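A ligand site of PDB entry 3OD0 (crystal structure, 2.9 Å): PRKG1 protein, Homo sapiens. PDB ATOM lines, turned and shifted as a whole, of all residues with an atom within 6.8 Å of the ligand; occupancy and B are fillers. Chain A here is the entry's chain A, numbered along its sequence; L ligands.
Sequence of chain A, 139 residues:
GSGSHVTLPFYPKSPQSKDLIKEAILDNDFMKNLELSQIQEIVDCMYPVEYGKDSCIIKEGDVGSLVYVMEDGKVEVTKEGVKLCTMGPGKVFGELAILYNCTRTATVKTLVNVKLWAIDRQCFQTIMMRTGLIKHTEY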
ATOM      1  N   ASN A  28      13.866 -10.767 -11.022  1.00  0.00           N
ATOM      2  CA  ASN A  28      13.637 -11.980 -11.782  1.00  0.00           C
ATOM      3  C   ASN A  28      12.289 -11.999 -12.524  1.00  0.00           C
ATOM      4  O   ASN A  28      11.238 -11.717 -11.923  1.00  0.00           O
ATOM      5  CB  ASN A  28      13.771 -13.203 -10.857  1.00  0.00           C
ATOM      6  CG  ASN A  28      13.295 -14.480 -11.498  1.00  0.00           C
ATOM      7  OD1 ASN A  28      12.202 -14.948 -11.211  1.00  0.00           O
ATOM      8  ND2 ASN A  28      14.115 -15.063 -12.358  1.00  0.00           N
ATOM      9  N   ILE A  58      24.237 -27.001 -11.018  1.00  0.00           N
ATOM     10  CA  ILE A  58      23.090 -27.553 -11.761  1.00  0.00           C
ATOM     11  C   ILE A  58      23.509 -28.147 -13.094  1.00  0.00           C
ATOM     12  O   ILE A  58      24.228 -27.513 -13.868  1.00  0.00           O
ATOM     13  CB  ILE A  58      22.100 -26.427 -12.095  1.00  0.00           C
ATOM     14  CG1 ILE A  58      21.519 -25.813 -10.829  1.00  0.00           C
ATOM     15  CG2 ILE A  58      20.968 -26.952 -12.965  1.00  0.00           C
ATOM     16  CD1 ILE A  58      20.430 -24.857 -11.117  1.00  0.00           C
ATOM     17  N   GLU A  60      22.185 -29.354 -16.707  1.00  0.00           N
ATOM     18  CA  GLU A  60      21.042 -29.342 -17.617  1.00  0.00           C
ATOM     19  C   GLU A  60      20.545 -30.765 -17.880  1.00  0.00           C
ATOM     20  O   GLU A  60      21.330 -31.713 -17.949  1.00  0.00           O
ATOM     21  CB  GLU A  60      21.395 -28.640 -18.928  1.00  0.00           C
ATOM     22  CG  GLU A  60      22.379 -29.385 -19.802  1.00  0.00           C
ATOM     23  CD  GLU A  60      22.892 -28.560 -20.975  1.00  0.00           C
ATOM     24  OE1 GLU A  60      23.947 -27.885 -20.840  1.00  0.00           O
ATOM     25  OE2 GLU A  60      22.238 -28.589 -22.045  1.00  0.00           O
ATOM     26  N   GLY A  64      15.026 -31.106 -11.078  1.00  0.00           N
ATOM     27  CA  GLY A  64      15.418 -29.987 -10.246  1.00  0.00           C
ATOM     28  C   GLY A  64      14.329 -29.304  -9.457  1.00  0.00           C
ATOM     29  O   GLY A  64      13.386 -28.773 -10.051  1.00  0.00           O
ATOM     30  N   LEU A  66      15.329 -27.194  -6.398  1.00  0.00           N
ATOM     31  CA  LEU A  66      15.834 -26.052  -5.663  1.00  0.00           C
ATOM     32  C   LEU A  66      15.975 -24.795  -6.498  1.00  0.00           C
ATOM     33  O   LEU A  66      16.333 -24.847  -7.665  1.00  0.00           O
ATOM     34  CB  LEU A  66      17.178 -26.379  -5.025  1.00  0.00           C
ATOM     35  CG  LEU A  66      17.247 -27.467  -3.959  1.00  0.00           C
ATOM     36  CD1 LEU A  66      18.697 -27.683  -3.604  1.00  0.00           C
ATOM     37  CD2 LEU A  66      16.442 -27.141  -2.704  1.00  0.00           C
ATOM     38  N   VAL A  77      26.703 -19.845 -17.074  1.00  0.00           N
ATOM     39  CA  VAL A  77      25.572 -20.628 -17.550  1.00  0.00           C
ATOM     40  C   VAL A  77      25.834 -21.117 -18.973  1.00  0.00           C
ATOM     41  O   VAL A  77      26.093 -20.322 -19.876  1.00  0.00           O
ATOM     42  CB  VAL A  77      24.314 -19.777 -17.554  1.00  0.00           C
ATOM     43  CG1 VAL A  77      23.112 -20.623 -17.940  1.00  0.00           C
ATOM     44  CG2 VAL A  77      24.100 -19.165 -16.196  1.00  0.00           C
ATOM     45  N   LYS A  79      24.472 -23.946 -22.135  1.00  0.00           N
ATOM     46  CA  LYS A  79      23.491 -24.878 -22.683  1.00  0.00           C
ATOM     47  C   LYS A  79      24.059 -25.566 -23.944  1.00  0.00           C
ATOM     48  O   LYS A  79      24.551 -24.903 -24.865  1.00  0.00           O
ATOM     49  CB  LYS A  79      22.150 -24.169 -22.973  1.00  0.00           C
ATOM     50  CG  LYS A  79      20.970 -25.106 -23.307  1.00  0.00           C
ATOM     51  CD  LYS A  79      19.600 -24.388 -23.371  1.00  0.00           C
ATOM     52  CE  LYS A  79      18.434 -25.390 -23.463  1.00  0.00           C
ATOM     53  NZ  LYS A  79      17.064 -24.754 -23.411  1.00  0.00           N
ATOM     54  N   LEU A  84      25.996 -18.804 -22.078  1.00  0.00           N
ATOM     55  CA  LEU A  84      24.816 -17.964 -22.268  1.00  0.00           C
ATOM     56  C   LEU A  84      25.044 -16.643 -21.536  1.00  0.00           C
ATOM     57  O   LEU A  84      24.634 -15.571 -22.003  1.00  0.00           O
ATOM     58  CB  LEU A  84      23.554 -18.657 -21.743  1.00  0.00           C
ATOM     59  CG  LEU A  84      23.191 -20.037 -22.304  1.00  0.00           C
ATOM     60  CD1 LEU A  84      21.793 -20.445 -21.872  1.00  0.00           C
ATOM     61  CD2 LEU A  84      23.316 -20.080 -23.827  1.00  0.00           C
ATOM     62  N   CYS A  85      25.699 -16.729 -20.398  1.00  0.00           N
ATOM     63  CA  CYS A  85      25.992 -15.542 -19.613  1.00  0.00           C
ATOM     64  C   CYS A  85      26.783 -15.953 -18.401  1.00  0.00           C
ATOM     65  O   CYS A  85      27.089 -17.133 -18.213  1.00  0.00           O
ATOM     66  CB  CYS A  85      24.691 -14.859 -19.172  1.00  0.00           C
ATOM     67  SG  CYS A  85      23.628 -15.905 -18.139  1.00  0.00           S
ATOM     68  N   MET A  87      26.698 -14.842 -14.022  1.00  0.00           N
ATOM     69  CA  MET A  87      25.814 -14.250 -13.038  1.00  0.00           C
ATOM     70  C   MET A  87      26.600 -13.965 -11.770  1.00  0.00           C
ATOM     71  O   MET A  87      27.369 -14.810 -11.305  1.00  0.00           O
ATOM     72  CB  MET A  87      24.646 -15.181 -12.717  1.00  0.00           C
ATOM     73  CG  MET A  87      23.417 -15.017 -13.604  1.00  0.00           C
ATOM     74  SD  MET A  87      22.174 -16.271 -13.229  1.00  0.00           S
ATOM     75  CE  MET A  87      23.092 -17.731 -13.672  1.00  0.00           C
ATOM     76  N   VAL A  92      18.747 -14.408  -9.185  1.00  0.00           N
ATOM     77  CA  VAL A  92      18.091 -15.700  -9.053  1.00  0.00           C
ATOM     78  C   VAL A  92      18.385 -16.618 -10.230  1.00  0.00           C
ATOM     79  O   VAL A  92      18.350 -16.200 -11.409  1.00  0.00           O
ATOM     80  CB  VAL A  92      16.563 -15.557  -9.035  1.00  0.00           C
ATOM     81  CG1 VAL A  92      15.909 -16.930  -9.134  1.00  0.00           C
ATOM     82  CG2 VAL A  92      16.087 -14.810  -7.812  1.00  0.00           C
ATOM     83  N   PHE A  93      18.648 -17.880  -9.927  1.00  0.00           N
ATOM     84  CA  PHE A  93      18.701 -18.902 -10.963  1.00  0.00           C
ATOM     85  C   PHE A  93      18.123 -20.205 -10.403  1.00  0.00           C
ATOM     86  O   PHE A  93      18.050 -20.378  -9.193  1.00  0.00           O
ATOM     87  CB  PHE A  93      20.118 -19.064 -11.507  1.00  0.00           C
ATOM     88  CG  PHE A  93      21.116 -19.524 -10.499  1.00  0.00           C
ATOM     89  CD1 PHE A  93      21.722 -18.611  -9.639  1.00  0.00           C
ATOM     90  CD2 PHE A  93      21.458 -20.866 -10.397  1.00  0.00           C
ATOM     91  CE1 PHE A  93      22.634 -19.031  -8.685  1.00  0.00           C
ATOM     92  CE2 PHE A  93      22.378 -21.293  -9.444  1.00  0.00           C
ATOM     93  CZ  PHE A  93      22.970 -20.366  -8.581  1.00  0.00           C
ATOM     94  N   GLY A  94      17.687 -21.095 -11.299  1.00  0.00           N
ATOM     95  CA  GLY A  94      17.080 -22.353 -10.884  1.00  0.00           C
ATOM     96  C   GLY A  94      15.566 -22.331 -10.840  1.00  0.00           C
ATOM     97  O   GLY A  94      14.929 -23.310 -10.447  1.00  0.00           O
ATOM     98  N   GLU A  95      14.979 -21.206 -11.255  1.00  0.00           N
ATOM     99  CA  GLU A  95      13.528 -21.049 -11.203  1.00  0.00           C
ATOM    100  C   GLU A  95      12.844 -21.792 -12.354  1.00  0.00           C
ATOM    101  O   GLU A  95      11.830 -22.468 -12.142  1.00  0.00           O
ATOM    102  CB  GLU A  95      13.170 -19.564 -11.163  1.00  0.00           C
ATOM    103  CG  GLU A  95      13.133 -18.837 -12.500  1.00  0.00           C
ATOM    104  CD  GLU A  95      14.503 -18.376 -12.983  1.00  0.00           C
ATOM    105  OE1 GLU A  95      15.510 -18.953 -12.542  1.00  0.00           O
ATOM    106  OE2 GLU A  95      14.562 -17.436 -13.825  1.00  0.00           O
ATOM    107  N   LEU A  96      13.434 -21.700 -13.541  1.00  0.00           N
ATOM    108  CA  LEU A  96      12.940 -22.345 -14.773  1.00  0.00           C
ATOM    109  C   LEU A  96      12.641 -23.851 -14.707  1.00  0.00           C
ATOM    110  O   LEU A  96      11.912 -24.372 -15.545  1.00  0.00           O
ATOM    111  CB  LEU A  96      13.890 -22.101 -15.947  1.00  0.00           C
ATOM    112  CG  LEU A  96      14.374 -20.676 -16.235  1.00  0.00           C
ATOM    113  CD1 LEU A  96      14.950 -20.552 -17.639  1.00  0.00           C
ATOM    114  CD2 LEU A  96      13.249 -19.701 -16.038  1.00  0.00           C
ATOM    115  N   ALA A  97      13.202 -24.579 -13.747  1.00  0.00           N
ATOM    116  CA  ALA A  97      12.980 -26.022 -13.738  1.00  0.00           C
ATOM    117  C   ALA A  97      11.475 -26.266 -13.772  1.00  0.00           C
ATOM    118  O   ALA A  97      10.967 -26.938 -14.673  1.00  0.00           O
ATOM    119  CB  ALA A  97      13.603 -26.682 -12.518  1.00  0.00           C
ATOM    120  N   ILE A  98      10.768 -25.691 -12.801  1.00  0.00           N
ATOM    121  CA  ILE A  98       9.348 -25.968 -12.607  1.00  0.00           C
ATOM    122  C   ILE A  98       8.530 -25.719 -13.873  1.00  0.00           C
ATOM    123  O   ILE A  98       7.667 -26.536 -14.243  1.00  0.00           O
ATOM    124  CB  ILE A  98       8.787 -25.138 -11.438  1.00  0.00           C
ATOM    125  CG1 ILE A  98       7.496 -25.763 -10.898  1.00  0.00           C
ATOM    126  CG2 ILE A  98       8.572 -23.698 -11.857  1.00  0.00           C
ATOM    127  CD1 ILE A  98       7.107 -25.302  -9.481  1.00  0.00           C
ATOM    128  N   TYR A 100       9.453 -25.981 -16.843  1.00  0.00           N
ATOM    129  CA  TYR A 100       9.774 -26.924 -17.902  1.00  0.00           C
ATOM    130  C   TYR A 100       9.762 -28.345 -17.377  1.00  0.00           C
ATOM    131  O   TYR A 100      10.604 -29.156 -17.744  1.00  0.00           O
ATOM    132  CB  TYR A 100      11.132 -26.631 -18.544  1.00  0.00           C
ATOM    133  CG  TYR A 100      11.202 -25.355 -19.334  1.00  0.00           C
ATOM    134  CD1 TYR A 100      11.284 -25.368 -20.728  1.00  0.00           C
ATOM    135  CD2 TYR A 100      11.205 -24.118 -18.692  1.00  0.00           C
ATOM    136  CE1 TYR A 100      11.369 -24.176 -21.465  1.00  0.00           C
ATOM    137  CE2 TYR A 100      11.290 -22.928 -19.420  1.00  0.00           C
ATOM    138  CZ  TYR A 100      11.365 -22.966 -20.798  1.00  0.00           C
ATOM    139  OH  TYR A 100      11.450 -21.769 -21.493  1.00  0.00           O
ATOM    140  N   THR A 103      12.548 -30.069 -15.053  1.00  0.00           N
ATOM    141  CA  THR A 103      13.839 -30.413 -15.625  1.00  0.00           C
ATOM    142  C   THR A 103      14.728 -29.161 -15.868  1.00  0.00           C
ATOM    143  O   THR A 103      14.320 -28.193 -16.521  1.00  0.00           O
ATOM    144  CB  THR A 103      13.715 -31.306 -16.900  1.00  0.00           C
ATOM    145  OG1 THR A 103      13.161 -30.546 -17.976  1.00  0.00           O
ATOM    146  CG2 THR A 103      12.847 -32.539 -16.643  1.00  0.00           C
ATOM    147  N   ARG A 104      15.929 -29.201 -15.292  1.00  0.00           N
ATOM    148  CA  ARG A 104      16.897 -28.135 -15.442  1.00  0.00           C
ATOM    149  C   ARG A 104      17.069 -27.790 -16.912  1.00  0.00           C
ATOM    150  O   ARG A 104      17.226 -28.690 -17.738  1.00  0.00           O
ATOM    151  CB  ARG A 104      18.235 -28.562 -14.846  1.00  0.00           C
ATOM    152  CG  ARG A 104      18.190 -28.808 -13.355  1.00  0.00           C
ATOM    153  CD  ARG A 104      17.719 -27.567 -12.651  1.00  0.00           C
ATOM    154  NE  ARG A 104      17.815 -27.687 -11.204  1.00  0.00           N
ATOM    155  CZ  ARG A 104      17.324 -26.785 -10.368  1.00  0.00           C
ATOM    156  NH1 ARG A 104      16.702 -25.712 -10.845  1.00  0.00           N
ATOM    157  NH2 ARG A 104      17.456 -26.954  -9.064  1.00  0.00           N
ATOM    158  N   THR A 105      17.060 -26.501 -17.261  1.00  0.00           N
ATOM    159  CA  THR A 105      17.131 -26.085 -18.665  1.00  0.00           C
ATOM    160  C   THR A 105      18.508 -25.642 -19.161  1.00  0.00           C
ATOM    161  O   THR A 105      18.694 -25.458 -20.359  1.00  0.00           O
ATOM    162  CB  THR A 105      16.092 -24.999 -18.986  1.00  0.00           C
ATOM    163  OG1 THR A 105      16.462 -23.771 -18.355  1.00  0.00           O
ATOM    164  CG2 THR A 105      14.722 -25.430 -18.507  1.00  0.00           C
ATOM    165  N   ALA A 106      19.452 -25.469 -18.244  1.00  0.00           N
ATOM    166  CA  ALA A 106      20.843 -25.125 -18.547  1.00  0.00           C
ATOM    167  C   ALA A 106      21.727 -25.576 -17.384  1.00  0.00           C
ATOM    168  O   ALA A 106      21.203 -25.843 -16.286  1.00  0.00           O
ATOM    169  CB  ALA A 106      21.002 -23.626 -18.789  1.00  0.00           C
ATOM    170  N   THR A 107      23.044 -25.690 -17.611  1.00  0.00           N
ATOM    171  CA  THR A 107      23.970 -26.066 -16.525  1.00  0.00           C
ATOM    172  C   THR A 107      24.638 -24.846 -15.916  1.00  0.00           C
ATOM    173  O   THR A 107      25.000 -23.910 -16.625  1.00  0.00           O
ATOM    174  CB  THR A 107      25.124 -26.941 -16.986  1.00  0.00           C
ATOM    175  OG1 THR A 107      26.109 -26.121 -17.607  1.00  0.00           O
ATOM    176  CG2 THR A 107      24.647 -28.041 -17.917  1.00  0.00           C
ATOM    177  N   VAL A 108      24.825 -24.885 -14.605  1.00  0.00           N
ATOM    178  CA  VAL A 108      25.465 -23.769 -13.916  1.00  0.00           C
ATOM    179  C   VAL A 108      26.761 -24.227 -13.245  1.00  0.00           C
ATOM    180  O   VAL A 108      26.722 -25.092 -12.376  1.00  0.00           O
ATOM    181  CB  VAL A 108      24.524 -23.178 -12.860  1.00  0.00           C
ATOM    182  CG1 VAL A 108      25.185 -22.027 -12.164  1.00  0.00           C
ATOM    183  CG2 VAL A 108      23.243 -22.736 -13.524  1.00  0.00           C
HETATM  184  P1  LIG L   1      16.945 -23.792 -14.310  1.00  0.00           P
HETATM  185  O1  LIG L   1      16.317 -24.388 -13.068  1.00  0.00           O
HETATM  186  O2  LIG L   1      16.500 -24.180 -15.692  1.00  0.00           O
HETATM  187  O3  LIG L   1      18.490 -24.186 -14.300  1.00  0.00           O
HETATM  188  C1  LIG L   1      19.420 -23.434 -15.079  1.00  0.00           C
HETATM  189  C2  LIG L   1      19.210 -21.986 -14.688  1.00  0.00           C
HETATM  190  O4  LIG L   1      20.053 -21.081 -15.373  1.00  0.00           O
HETATM  191  C3  LIG L   1      17.835 -21.521 -15.092  1.00  0.00           C
HETATM  192  O5  LIG L   1      16.912 -22.180 -14.242  1.00  0.00           O
HETATM  193  C4  LIG L   1      17.972 -20.019 -14.975  1.00  0.00           C
HETATM  194  O6  LIG L   1      17.625 -19.562 -13.672  1.00  0.00           O
HETATM  195  C5  LIG L   1      19.463 -19.783 -15.240  1.00  0.00           C
HETATM  196  N1  LIG L   1      19.680 -19.003 -16.484  1.00  0.00           N
HETATM  197  C6  LIG L   1      20.265 -17.794 -16.635  1.00  0.00           C
HETATM  198  N2  LIG L   1      20.294 -17.388 -17.928  1.00  0.00           N
HETATM  199  C7  LIG L   1      19.710 -18.369 -18.639  1.00  0.00           C
HETATM  200  C8  LIG L   1      19.391 -18.617 -20.063  1.00  0.00           C
HETATM  201  O7  LIG L   1      19.698 -17.765 -20.924  1.00  0.00           O
HETATM  202  N3  LIG L   1      18.771 -19.776 -20.383  1.00  0.00           N
HETATM  203  C9  LIG L   1      18.443 -20.708 -19.447  1.00  0.00           C
HETATM  204  N4  LIG L   1      17.817 -21.866 -19.808  1.00  0.00           N
HETATM  205  N5  LIG L   1      18.714 -20.548 -18.124  1.00  0.00           N
HETATM  206  C10 LIG L   1      19.333 -19.430 -17.680  1.00  0.00           C
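OE1 of Glu 95 is in hydrogen-bond range of O6 of the ligand, 2.5 Å away. The guanidinium group (NH1) of Arg 104 lies within salt-bridge range of an oxygen (O1) of the ligand. An oxygen (O2) of the ligand lies within hydrogen-bond range of the backbone NH (N) of Thr 105, 2.9 Å away. OG1 of Thr 105 is in hydrogen-bond range of O2 of the ligand, at 2.7 Å. N of Gly 94 sits at hydrogen-bond distance from O6 of the ligand (2.8 Å). N of Ala 97 is in hydrogen-bond range of O1 of the ligand (3.2 Å). A nitrogen (N2) of the ligand is in hydrogen-bond range of the side-chain sulfur of Cys 85, 3.7 Å away.
The side-chain amide nitrogen (ND2) of Asn 28 sits at hydrogen-bond distance from the side-chain carboxylate (OE2) of Glu 95 (2.8 Å). The backbone carbonyl oxygen (O) of Gly 94 sits at hydrogen-bond distance from the guanidinium group (NH1) of Arg 104, 3.0 Å away. NH2 of Arg 104 lies within hydrogen-bond range of O of Leu 66 (2.8 Å). The backbone NH of Leu 84 sits at hydrogen-bond distance from the backbone carbonyl oxygen of Val 77 (2.7 Å). The backbone carbonyl oxygen (O) of Cys 85 sits at hydrogen-bond distance from the backbone NH (N) of Val 77 (3.0 Å). The backbone NH (N) of Val 108 is in hydrogen-bond range of the backbone carbonyl oxygen (O) of Ile 58 (2.8 Å).
Ile 58 touches the ligand. CG1 of Val 77 touches C10 of the ligand, 3.97 Å away. CD1 of Leu 84 touches N3 of the ligand, 3.4 Å away. Phe 93 touches the ligand (CA to O6, 3.0 Å). CB of Leu 96 touches O2 of the ligand (3.3 Å). Ala 106 touches the ligand (O to C1, 3.2 Å). Hydrophobic or aromatic side chains that line the ligand: Ile 58, Val 77, Leu 84, Phe 93, Leu 96, Ala 97 and Ala 106. The nearest printed residue that does not touch the ligand is Val 108 (4.04 Å).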
